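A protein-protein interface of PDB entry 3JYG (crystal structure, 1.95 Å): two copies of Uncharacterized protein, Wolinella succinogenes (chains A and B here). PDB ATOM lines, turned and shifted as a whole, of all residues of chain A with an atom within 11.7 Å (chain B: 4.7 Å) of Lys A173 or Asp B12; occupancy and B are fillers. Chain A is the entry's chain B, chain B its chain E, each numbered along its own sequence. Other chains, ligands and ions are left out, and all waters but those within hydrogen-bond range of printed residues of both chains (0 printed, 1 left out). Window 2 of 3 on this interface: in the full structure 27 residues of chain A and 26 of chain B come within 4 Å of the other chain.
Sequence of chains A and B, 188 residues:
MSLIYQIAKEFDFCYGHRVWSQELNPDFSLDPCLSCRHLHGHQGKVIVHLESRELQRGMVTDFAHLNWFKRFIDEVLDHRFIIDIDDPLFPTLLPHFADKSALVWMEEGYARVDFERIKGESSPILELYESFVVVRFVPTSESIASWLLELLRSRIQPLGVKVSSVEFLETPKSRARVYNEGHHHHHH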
ATOM      1  N   TYR A  15       7.029  38.780  15.356  1.00  0.00           N
ATOM      2  CA  TYR A  15       6.786  40.188  15.052  1.00  0.00           C
ATOM      3  C   TYR A  15       5.285  40.455  14.995  1.00  0.00           C
ATOM      4  O   TYR A  15       4.499  39.532  14.818  1.00  0.00           O
ATOM      5  CB  TYR A  15       7.469  40.600  13.684  1.00  0.00           C
ATOM      6  CG  TYR A  15       6.916  39.858  12.470  1.00  0.00           C
ATOM      7  CD1 TYR A  15       7.176  38.496  12.266  1.00  0.00           C
ATOM      8  CD2 TYR A  15       6.138  40.512  11.510  1.00  0.00           C
ATOM      9  CE1 TYR A  15       6.654  37.814  11.155  1.00  0.00           C
ATOM     10  CE2 TYR A  15       5.608  39.828  10.391  1.00  0.00           C
ATOM     11  CZ  TYR A  15       5.866  38.480  10.222  1.00  0.00           C
ATOM     12  OH  TYR A  15       5.353  37.802   9.100  1.00  0.00           O
ATOM     13  N   HIS A  42       2.921  37.282  13.901  1.00  0.00           N
ATOM     14  CA  HIS A  42       3.285  35.993  13.374  1.00  0.00           C
ATOM     15  C   HIS A  42       4.563  35.490  13.997  1.00  0.00           C
ATOM     16  O   HIS A  42       5.361  36.271  14.595  1.00  0.00           O
ATOM     17  CB  HIS A  42       3.561  36.116  11.874  1.00  0.00           C
ATOM     18  CG  HIS A  42       2.352  36.371  11.064  1.00  0.00           C
ATOM     19  ND1 HIS A  42       1.340  35.440  10.934  1.00  0.00           N
ATOM     20  CD2 HIS A  42       2.001  37.436  10.294  1.00  0.00           C
ATOM     21  CE1 HIS A  42       0.405  35.931  10.124  1.00  0.00           C
ATOM     22  NE2 HIS A  42       0.778  37.139   9.737  1.00  0.00           N
ATOM     23  N   GLN A  43       4.745  34.190  13.870  1.00  0.00           N
ATOM     24  CA  GLN A  43       6.067  33.576  14.036  1.00  0.00           C
ATOM     25  C   GLN A  43       6.686  33.409  12.650  1.00  0.00           C
ATOM     26  O   GLN A  43       6.200  32.634  11.850  1.00  0.00           O
ATOM     27  CB  GLN A  43       5.961  32.249  14.766  1.00  0.00           C
ATOM     28  CG  GLN A  43       7.236  31.382  14.725  1.00  0.00           C
ATOM     29  CD  GLN A  43       8.208  31.654  15.852  1.00  0.00           C
ATOM     30  OE1 GLN A  43       7.866  32.313  16.833  1.00  0.00           O
ATOM     31  NE2 GLN A  43       9.425  31.114  15.740  1.00  0.00           N
ATOM     32  N   GLY A  44       7.711  34.183  12.360  1.00  0.00           N
ATOM     33  CA  GLY A  44       8.305  34.194  11.013  1.00  0.00           C
ATOM     34  C   GLY A  44       9.488  33.238  10.905  1.00  0.00           C
ATOM     35  O   GLY A  44      10.146  32.980  11.911  1.00  0.00           O
ATOM     36  N   LYS A  45       9.752  32.707   9.706  1.00  0.00           N
ATOM     37  CA  LYS A  45      10.963  31.958   9.495  1.00  0.00           C
ATOM     38  C   LYS A  45      11.471  32.390   8.143  1.00  0.00           C
ATOM     39  O   LYS A  45      10.705  32.366   7.173  1.00  0.00           O
ATOM     40  CB  LYS A  45      10.706  30.428   9.499  1.00  0.00           C
ATOM     41  CG  LYS A  45      11.913  29.561   9.048  1.00  0.00           C
ATOM     42  CD  LYS A  45      11.470  28.101   8.789  1.00  0.00           C
ATOM     43  CE  LYS A  45      10.949  27.443  10.097  1.00  0.00           C
ATOM     44  NZ  LYS A  45      11.943  27.461  11.240  1.00  0.00           N
ATOM     45  N   ILE A  47      14.402  31.564   5.311  1.00  0.00           N
ATOM     46  CA  ILE A  47      15.248  30.490   4.873  1.00  0.00           C
ATOM     47  C   ILE A  47      16.034  31.070   3.702  1.00  0.00           C
ATOM     48  O   ILE A  47      15.452  31.446   2.693  1.00  0.00           O
ATOM     49  CB  ILE A  47      14.476  29.248   4.360  1.00  0.00           C
ATOM     50  CG1 ILE A  47      13.423  28.792   5.407  1.00  0.00           C
ATOM     51  CG2 ILE A  47      15.501  28.146   3.953  1.00  0.00           C
ATOM     52  CD1 ILE A  47      12.770  27.375   5.179  1.00  0.00           C
ATOM     53  N   SER A 141       4.599  38.800   3.389  1.00  0.00           N
ATOM     54  CA  SER A 141       5.656  37.795   3.286  1.00  0.00           C
ATOM     55  C   SER A 141       6.474  37.962   2.042  1.00  0.00           C
ATOM     56  O   SER A 141       7.666  37.848   2.122  1.00  0.00           O
ATOM     57  CB  SER A 141       5.084  36.387   3.298  1.00  0.00           C
ATOM     58  OG  SER A 141       4.247  36.159   4.424  1.00  0.00           O
ATOM     59  N   GLU A 167      13.237  32.333   1.248  1.00  0.00           N
ATOM     60  CA  GLU A 167      11.880  32.016   1.655  1.00  0.00           C
ATOM     61  C   GLU A 167      11.526  32.780   2.909  1.00  0.00           C
ATOM     62  O   GLU A 167      12.399  33.037   3.733  1.00  0.00           O
ATOM     63  CB  GLU A 167      11.752  30.518   1.980  1.00  0.00           C
ATOM     64  CG  GLU A 167      12.081  29.616   0.789  1.00  0.00           C
ATOM     65  CD  GLU A 167      11.854  28.170   1.155  1.00  0.00           C
ATOM     66  OE1 GLU A 167      12.849  27.452   1.351  1.00  0.00           O
ATOM     67  OE2 GLU A 167      10.683  27.799   1.329  1.00  0.00           O
ATOM     68  N   PHE A 168      10.267  33.178   3.026  1.00  0.00           N
ATOM     69  CA  PHE A 168       9.751  33.716   4.283  1.00  0.00           C
ATOM     70  C   PHE A 168       8.458  33.025   4.640  1.00  0.00           C
ATOM     71  O   PHE A 168       7.487  33.182   3.933  1.00  0.00           O
ATOM     72  CB  PHE A 168       9.525  35.209   4.163  1.00  0.00           C
ATOM     73  CG  PHE A 168       9.143  35.859   5.481  1.00  0.00           C
ATOM     74  CD1 PHE A 168      10.112  36.149   6.441  1.00  0.00           C
ATOM     75  CD2 PHE A 168       7.827  36.087   5.783  1.00  0.00           C
ATOM     76  CE1 PHE A 168       9.756  36.717   7.686  1.00  0.00           C
ATOM     77  CE2 PHE A 168       7.455  36.618   7.016  1.00  0.00           C
ATOM     78  CZ  PHE A 168       8.426  36.968   7.956  1.00  0.00           C
ATOM     79  N   LEU A 169       8.448  32.224   5.722  1.00  0.00           N
ATOM     80  CA  LEU A 169       7.242  31.510   6.155  1.00  0.00           C
ATOM     81  C   LEU A 169       6.464  32.377   7.137  1.00  0.00           C
ATOM     82  O   LEU A 169       6.991  32.735   8.174  1.00  0.00           O
ATOM     83  CB  LEU A 169       7.581  30.135   6.809  1.00  0.00           C
ATOM     84  CG  LEU A 169       8.199  28.997   5.963  1.00  0.00           C
ATOM     85  CD1 LEU A 169       9.561  29.319   5.396  1.00  0.00           C
ATOM     86  CD2 LEU A 169       8.262  27.691   6.765  1.00  0.00           C
ATOM     87  N   GLU A 170       5.226  32.706   6.789  1.00  0.00           N
ATOM     88  CA  GLU A 170       4.400  33.588   7.581  1.00  0.00           C
ATOM     89  C   GLU A 170       3.689  32.770   8.659  1.00  0.00           C
ATOM     90  O   GLU A 170       3.467  33.239   9.781  1.00  0.00           O
ATOM     91  CB  GLU A 170       3.442  34.345   6.652  1.00  0.00           C
ATOM     92  CG  GLU A 170       2.110  34.807   7.232  1.00  0.00           C
ATOM     93  CD  GLU A 170       1.145  35.333   6.190  1.00  0.00           C
ATOM     94  OE1 GLU A 170       1.625  35.844   5.148  1.00  0.00           O
ATOM     95  OE2 GLU A 170      -0.086  35.256   6.411  1.00  0.00           O
ATOM     96  N   THR A 171       3.336  31.547   8.299  1.00  0.00           N
ATOM     97  CA  THR A 171       2.825  30.567   9.227  1.00  0.00           C
ATOM     98  C   THR A 171       3.439  29.232   8.792  1.00  0.00           C
ATOM     99  O   THR A 171       4.038  29.148   7.711  1.00  0.00           O
ATOM    100  CB  THR A 171       1.267  30.462   9.192  1.00  0.00           C
ATOM    101  OG1 THR A 171       0.872  29.678   8.052  1.00  0.00           O
ATOM    102  CG2 THR A 171       0.579  31.845   9.105  1.00  0.00           C
ATOM    103  N   PRO A 172       3.312  28.192   9.631  1.00  0.00           N
ATOM    104  CA  PRO A 172       3.812  26.880   9.189  1.00  0.00           C
ATOM    105  C   PRO A 172       3.132  26.382   7.912  1.00  0.00           C
ATOM    106  O   PRO A 172       3.716  25.589   7.206  1.00  0.00           O
ATOM    107  CB  PRO A 172       3.452  25.941  10.353  1.00  0.00           C
ATOM    108  CG  PRO A 172       3.091  26.851  11.525  1.00  0.00           C
ATOM    109  CD  PRO A 172       2.557  28.113  10.905  1.00  0.00           C
ATOM    110  N   LYS A 173       1.920  26.827   7.617  1.00  0.00           N
ATOM    111  CA  LYS A 173       1.248  26.369   6.394  1.00  0.00           C
ATOM    112  C   LYS A 173       1.322  27.293   5.184  1.00  0.00           C
ATOM    113  O   LYS A 173       0.864  26.902   4.119  1.00  0.00           O
ATOM    114  CB  LYS A 173      -0.209  26.030   6.653  1.00  0.00           C
ATOM    115  CG  LYS A 173      -0.360  24.741   7.446  1.00  0.00           C
ATOM    116  CD  LYS A 173      -1.809  24.302   7.467  1.00  0.00           C
ATOM    117  CE  LYS A 173      -2.006  23.242   8.523  1.00  0.00           C
ATOM    118  NZ  LYS A 173      -1.597  23.821   9.856  1.00  0.00           N
ATOM    119  N   SER A 174       1.872  28.495   5.335  1.00  0.00           N
ATOM    120  CA  SER A 174       1.915  29.443   4.209  1.00  0.00           C
ATOM    121  C   SER A 174       3.229  30.223   4.140  1.00  0.00           C
ATOM    122  O   SER A 174       3.773  30.628   5.170  1.00  0.00           O
ATOM    123  CB  SER A 174       0.743  30.378   4.320  1.00  0.00           C
ATOM    124  OG  SER A 174       1.003  31.250   5.387  1.00  0.00           O
ATOM    125  N   ARG A 175       3.753  30.404   2.922  1.00  0.00           N
ATOM    126  CA  ARG A 175       5.071  31.003   2.762  1.00  0.00           C
ATOM    127  C   ARG A 175       5.248  31.636   1.408  1.00  0.00           C
ATOM    128  O   ARG A 175       4.508  31.365   0.480  1.00  0.00           O
ATOM    129  CB  ARG A 175       6.200  29.991   3.048  1.00  0.00           C
ATOM    130  CG  ARG A 175       6.180  28.661   2.237  1.00  0.00           C
ATOM    131  CD  ARG A 175       6.783  27.548   3.114  1.00  0.00           C
ATOM    132  NE  ARG A 175       6.693  26.207   2.541  1.00  0.00           N
ATOM    133  CZ  ARG A 175       5.552  25.603   2.214  1.00  0.00           C
ATOM    134  NH1 ARG A 175       4.387  26.231   2.379  1.00  0.00           N
ATOM    135  NH2 ARG A 175       5.581  24.378   1.720  1.00  0.00           N
ATOM    136  N   ALA A 176       6.251  32.488   1.325  1.00  0.00           N
ATOM    137  CA  ALA A 176       6.599  33.191   0.114  1.00  0.00           C
ATOM    138  C   ALA A 176       8.009  32.764  -0.260  1.00  0.00           C
ATOM    139  O   ALA A 176       8.778  32.364   0.584  1.00  0.00           O
ATOM    140  CB  ALA A 176       6.521  34.725   0.372  1.00  0.00           C
ATOM    141  N   ARG A 177       8.350  32.832  -1.532  1.00  0.00           N
ATOM    142  CA  ARG A 177       9.718  32.588  -1.951  1.00  0.00           C
ATOM    143  C   ARG A 177      10.031  33.585  -3.083  1.00  0.00           C
ATOM    144  O   ARG A 177       9.211  33.813  -3.973  1.00  0.00           O
ATOM    145  CB  ARG A 177       9.858  31.150  -2.458  1.00  0.00           C
ATOM    146  CG  ARG A 177      11.261  30.741  -2.923  1.00  0.00           C
ATOM    147  CD  ARG A 177      11.441  29.226  -2.864  1.00  0.00           C
ATOM    148  NE  ARG A 177      12.839  28.803  -2.855  1.00  0.00           N
ATOM    149  CZ  ARG A 177      13.209  27.541  -2.661  1.00  0.00           C
ATOM    150  NH1 ARG A 177      12.272  26.618  -2.457  1.00  0.00           N
ATOM    151  NH2 ARG A 177      14.496  27.183  -2.674  1.00  0.00           N
ATOM    152  N   ALA B   8       3.376  29.547  -1.477  1.00  0.00           N
ATOM    153  CA  ALA B   8       2.923  28.143  -1.352  1.00  0.00           C
ATOM    154  C   ALA B   8       2.012  28.056  -0.143  1.00  0.00           C
ATOM    155  O   ALA B   8       2.292  28.690   0.865  1.00  0.00           O
ATOM    156  CB  ALA B   8       4.082  27.223  -1.162  1.00  0.00           C
ATOM    157  N   LYS B   9       0.959  27.246  -0.218  1.00  0.00           N
ATOM    158  CA  LYS B   9       0.081  27.049   0.960  1.00  0.00           C
ATOM    159  C   LYS B   9      -0.277  25.552   1.043  1.00  0.00           C
ATOM    160  O   LYS B   9      -0.457  24.894   0.001  1.00  0.00           O
ATOM    161  CB  LYS B   9      -1.190  27.910   0.853  1.00  0.00           C
ATOM    162  CG  LYS B   9      -2.104  27.654   2.067  1.00  0.00           C
ATOM    163  CD  LYS B   9      -2.959  28.793   2.479  1.00  0.00           C
ATOM    164  CE  LYS B   9      -3.828  28.353   3.664  1.00  0.00           C
ATOM    165  NZ  LYS B   9      -4.941  29.371   3.844  1.00  0.00           N
ATOM    166  N   GLU B  10      -0.259  25.019   2.272  1.00  0.00           N
ATOM    167  CA  GLU B  10      -0.589  23.616   2.605  1.00  0.00           C
ATOM    168  C   GLU B  10      -2.066  23.369   2.961  1.00  0.00           C
ATOM    169  O   GLU B  10      -2.707  24.171   3.668  1.00  0.00           O
ATOM    170  CB  GLU B  10       0.224  23.207   3.808  1.00  0.00           C
ATOM    171  CG  GLU B  10       1.673  23.476   3.682  1.00  0.00           C
ATOM    172  CD  GLU B  10       2.473  22.826   4.775  1.00  0.00           C
ATOM    173  OE1 GLU B  10       1.868  22.335   5.731  1.00  0.00           O
ATOM    174  OE2 GLU B  10       3.715  22.823   4.683  1.00  0.00           O
ATOM    175  N   PHE B  11      -2.590  22.227   2.522  1.00  0.00           N
ATOM    176  CA  PHE B  11      -3.965  21.826   2.814  1.00  0.00           C
ATOM    177  C   PHE B  11      -3.915  20.361   3.235  1.00  0.00           C
ATOM    178  O   PHE B  11      -3.337  19.544   2.508  1.00  0.00           O
ATOM    179  CB  PHE B  11      -4.838  21.970   1.545  1.00  0.00           C
ATOM    180  CG  PHE B  11      -4.793  23.338   0.978  1.00  0.00           C
ATOM    181  CD1 PHE B  11      -3.810  23.699   0.050  1.00  0.00           C
ATOM    182  CD2 PHE B  11      -5.686  24.309   1.439  1.00  0.00           C
ATOM    183  CE1 PHE B  11      -3.722  25.005  -0.403  1.00  0.00           C
ATOM    184  CE2 PHE B  11      -5.605  25.610   0.972  1.00  0.00           C
ATOM    185  CZ  PHE B  11      -4.626  25.940   0.032  1.00  0.00           C
ATOM    186  N   ASP B  12      -4.518  20.044   4.382  1.00  0.00           N
ATOM    187  CA  ASP B  12      -4.476  18.670   4.966  1.00  0.00           C
ATOM    188  C   ASP B  12      -5.819  17.953   4.820  1.00  0.00           C
ATOM    189  O   ASP B  12      -6.882  18.579   4.890  1.00  0.00           O
ATOM    190  CB  ASP B  12      -4.158  18.719   6.457  1.00  0.00           C
ATOM    191  CG  ASP B  12      -2.775  19.235   6.758  1.00  0.00           C
ATOM    192  OD1 ASP B  12      -2.648  19.891   7.811  1.00  0.00           O
ATOM    193  OD2 ASP B  12      -1.806  18.988   6.004  1.00  0.00           O
ATOM    194  N   PHE B  13      -5.773  16.636   4.631  1.00  0.00           N
ATOM    195  CA  PHE B  13      -7.000  15.794   4.696  1.00  0.00           C
ATOM    196  C   PHE B  13      -6.617  14.341   4.907  1.00  0.00           C
ATOM    197  O   PHE B  13      -5.466  13.975   4.646  1.00  0.00           O
ATOM    198  CB  PHE B  13      -7.911  15.967   3.447  1.00  0.00           C
ATOM    199  CG  PHE B  13      -7.351  15.376   2.146  1.00  0.00           C
ATOM    200  CD1 PHE B  13      -6.339  16.031   1.422  1.00  0.00           C
ATOM    201  CD2 PHE B  13      -7.860  14.190   1.638  1.00  0.00           C
ATOM    202  CE1 PHE B  13      -5.836  15.474   0.193  1.00  0.00           C
ATOM    203  CE2 PHE B  13      -7.384  13.633   0.421  1.00  0.00           C
ATOM    204  CZ  PHE B  13      -6.399  14.284  -0.309  1.00  0.00           C
ATOM    205  N   GLN B  43      -2.759  10.144   5.802  1.00  0.00           N
ATOM    206  CA  GLN B  43      -2.841  11.587   6.070  1.00  0.00           C
ATOM    207  C   GLN B  43      -2.178  12.296   4.869  1.00  0.00           C
ATOM    208  O   GLN B  43      -0.990  12.074   4.594  1.00  0.00           O
ATOM    209  CB  GLN B  43      -2.069  11.888   7.372  1.00  0.00           C
ATOM    210  CG  GLN B  43      -1.973  13.400   7.730  1.00  0.00           C
ATOM    211  CD  GLN B  43      -3.326  13.997   8.058  1.00  0.00           C
ATOM    212  OE1 GLN B  43      -4.199  13.303   8.580  1.00  0.00           O
ATOM    213  NE2 GLN B  43      -3.501  15.295   7.803  1.00  0.00           N
ATOM    214  N   GLY B  44      -2.957  13.060   4.110  1.00  0.00           N
ATOM    215  CA  GLY B  44      -2.468  13.699   2.884  1.00  0.00           C
ATOM    216  C   GLY B  44      -2.223  15.161   3.142  1.00  0.00           C
ATOM    217  O   GLY B  44      -2.906  15.763   3.994  1.00  0.00           O
ATOM    218  N   LYS B  45      -1.185  15.709   2.520  1.00  0.00           N
ATOM    219  CA  LYS B  45      -0.971  17.146   2.522  1.00  0.00           C
ATOM    220  C   LYS B  45      -0.809  17.640   1.065  1.00  0.00           C
ATOM    221  O   LYS B  45       0.056  17.150   0.358  1.00  0.00           O
ATOM    222  CB  LYS B  45       0.294  17.474   3.319  1.00  0.00           C
ATOM    223  CG  LYS B  45       0.554  18.961   3.446  1.00  0.00           C
ATOM    224  CD  LYS B  45       1.918  19.244   4.214  1.00  0.00           C
ATOM    225  CE  LYS B  45       1.811  18.878   5.717  1.00  0.00           C
ATOM    226  NZ  LYS B  45       0.900  19.830   6.458  1.00  0.00           N
ATOM    227  N   ILE B  73     -11.228  20.600  -0.712  1.00  0.00           N
ATOM    228  CA  ILE B  73     -10.562  19.562   0.101  1.00  0.00           C
ATOM    229  C   ILE B  73     -11.411  19.092   1.316  1.00  0.00           C
ATOM    230  O   ILE B  73     -11.604  17.862   1.565  1.00  0.00           O
ATOM    231  CB  ILE B  73      -9.147  20.021   0.601  1.00  0.00           C
ATOM    232  CG1 ILE B  73      -8.163  20.335  -0.567  1.00  0.00           C
ATOM    233  CG2 ILE B  73      -8.497  18.927   1.395  1.00  0.00           C
ATOM    234  CD1 ILE B  73      -8.190  19.311  -1.623  1.00  0.00           C
ATOM    235  N   ASP B  74     -11.877  20.059   2.091  1.00  0.00           N
ATOM    236  CA  ASP B  74     -12.628  19.765   3.298  1.00  0.00           C
ATOM    237  C   ASP B  74     -13.963  19.065   3.004  1.00  0.00           C
ATOM    238  O   ASP B  74     -14.394  18.172   3.716  1.00  0.00           O
ATOM    239  CB  ASP B  74     -12.895  21.074   4.066  1.00  0.00           C
ATOM    240  CG  ASP B  74     -11.622  21.646   4.727  1.00  0.00           C
ATOM    241  OD1 ASP B  74     -10.592  20.909   4.786  1.00  0.00           O
ATOM    242  OD2 ASP B  74     -11.635  22.838   5.155  1.00  0.00           O
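The side-chain carboxylate (OE2) of Glu B10 is in salt-bridge range of the guanidinium group (NH2) of Arg A175 (3.8 Å).
O of Lys A173 lies within hydrogen-bond range of N of Glu B10 (2.9 Å).
O of Arg A175 is in hydrogen-bond range of N of Ala B8 (2.9 Å).
OG1 of Thr A171 lies within hydrogen-bond range of OG of Ser A174 (3.1 Å).
OD2 of Asp B12 is in salt-bridge range of NZ of Lys B45 (2.9 Å).
The side-chain hydroxyl (OG1) of Thr A171 is in hydrogen-bond range of the backbone NH (N) of Lys A173 (3.1 Å).
The side-chain carboxylate (OE1) of Glu B10 is in salt-bridge range of the side-chain amino group (NZ) of Lys B45.
OE2 of Glu B10 touches O of Pro A172, at 3.7 Å.
O of Ala B8 touches O of Lys A173 (3.98 Å).
O of Lys A173 touches CA of Lys B9, 3.3 Å away.
Lys A173 touches Asp B12.
Ala B8 touches Ser A174 (O to CA, 3.4 Å).
Gln A43 touches none of the printed residues of chain B.
Phe A168 touches none of the printed residues of chain B.
Of the printed residues of chain B, Pro A172 touches Glu B10.
Printed residues of chain B within 4 Å of Lys A173: Ala B8, Lys B9, Glu B10 and Asp B12.
Of the printed residues of chain B, Ser A174 touches Ala B8.
Of the printed residues of chain B, Arg A175 touches Ala B8 (2.9 Å) and Glu B10 (3.8 Å).
Of the printed residues of chain A, Ala B8 touches Lys A173 (3.98 Å), Ser A174 (3.4 Å) and Arg A175 (2.9 Å).
Of the printed residues of chain A, Glu B10 touches Pro A172, Lys A173 and Arg A175.
Asp B12 touches one residue of chain A.
No residue of chain A comes within 4 Å of Phe B13.
No residue of chain A comes within 4 Å of Ile B73.
No residue of chain A comes within 4 Å of Asp B74.
The nearest printed residue of chain B that does not touch Lys A173 is Lys B45 (4.9 Å).
The nearest residue of chain A that does not touch Asp B12 is Pro A172 (8.6 Å).
Of the 18 printed residues of chain A, 4 touch a printed residue of chain B.
Among the printed residues, 8 pairs touch across the chains.
Positions printed for both chains: 43, 44 and 45.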
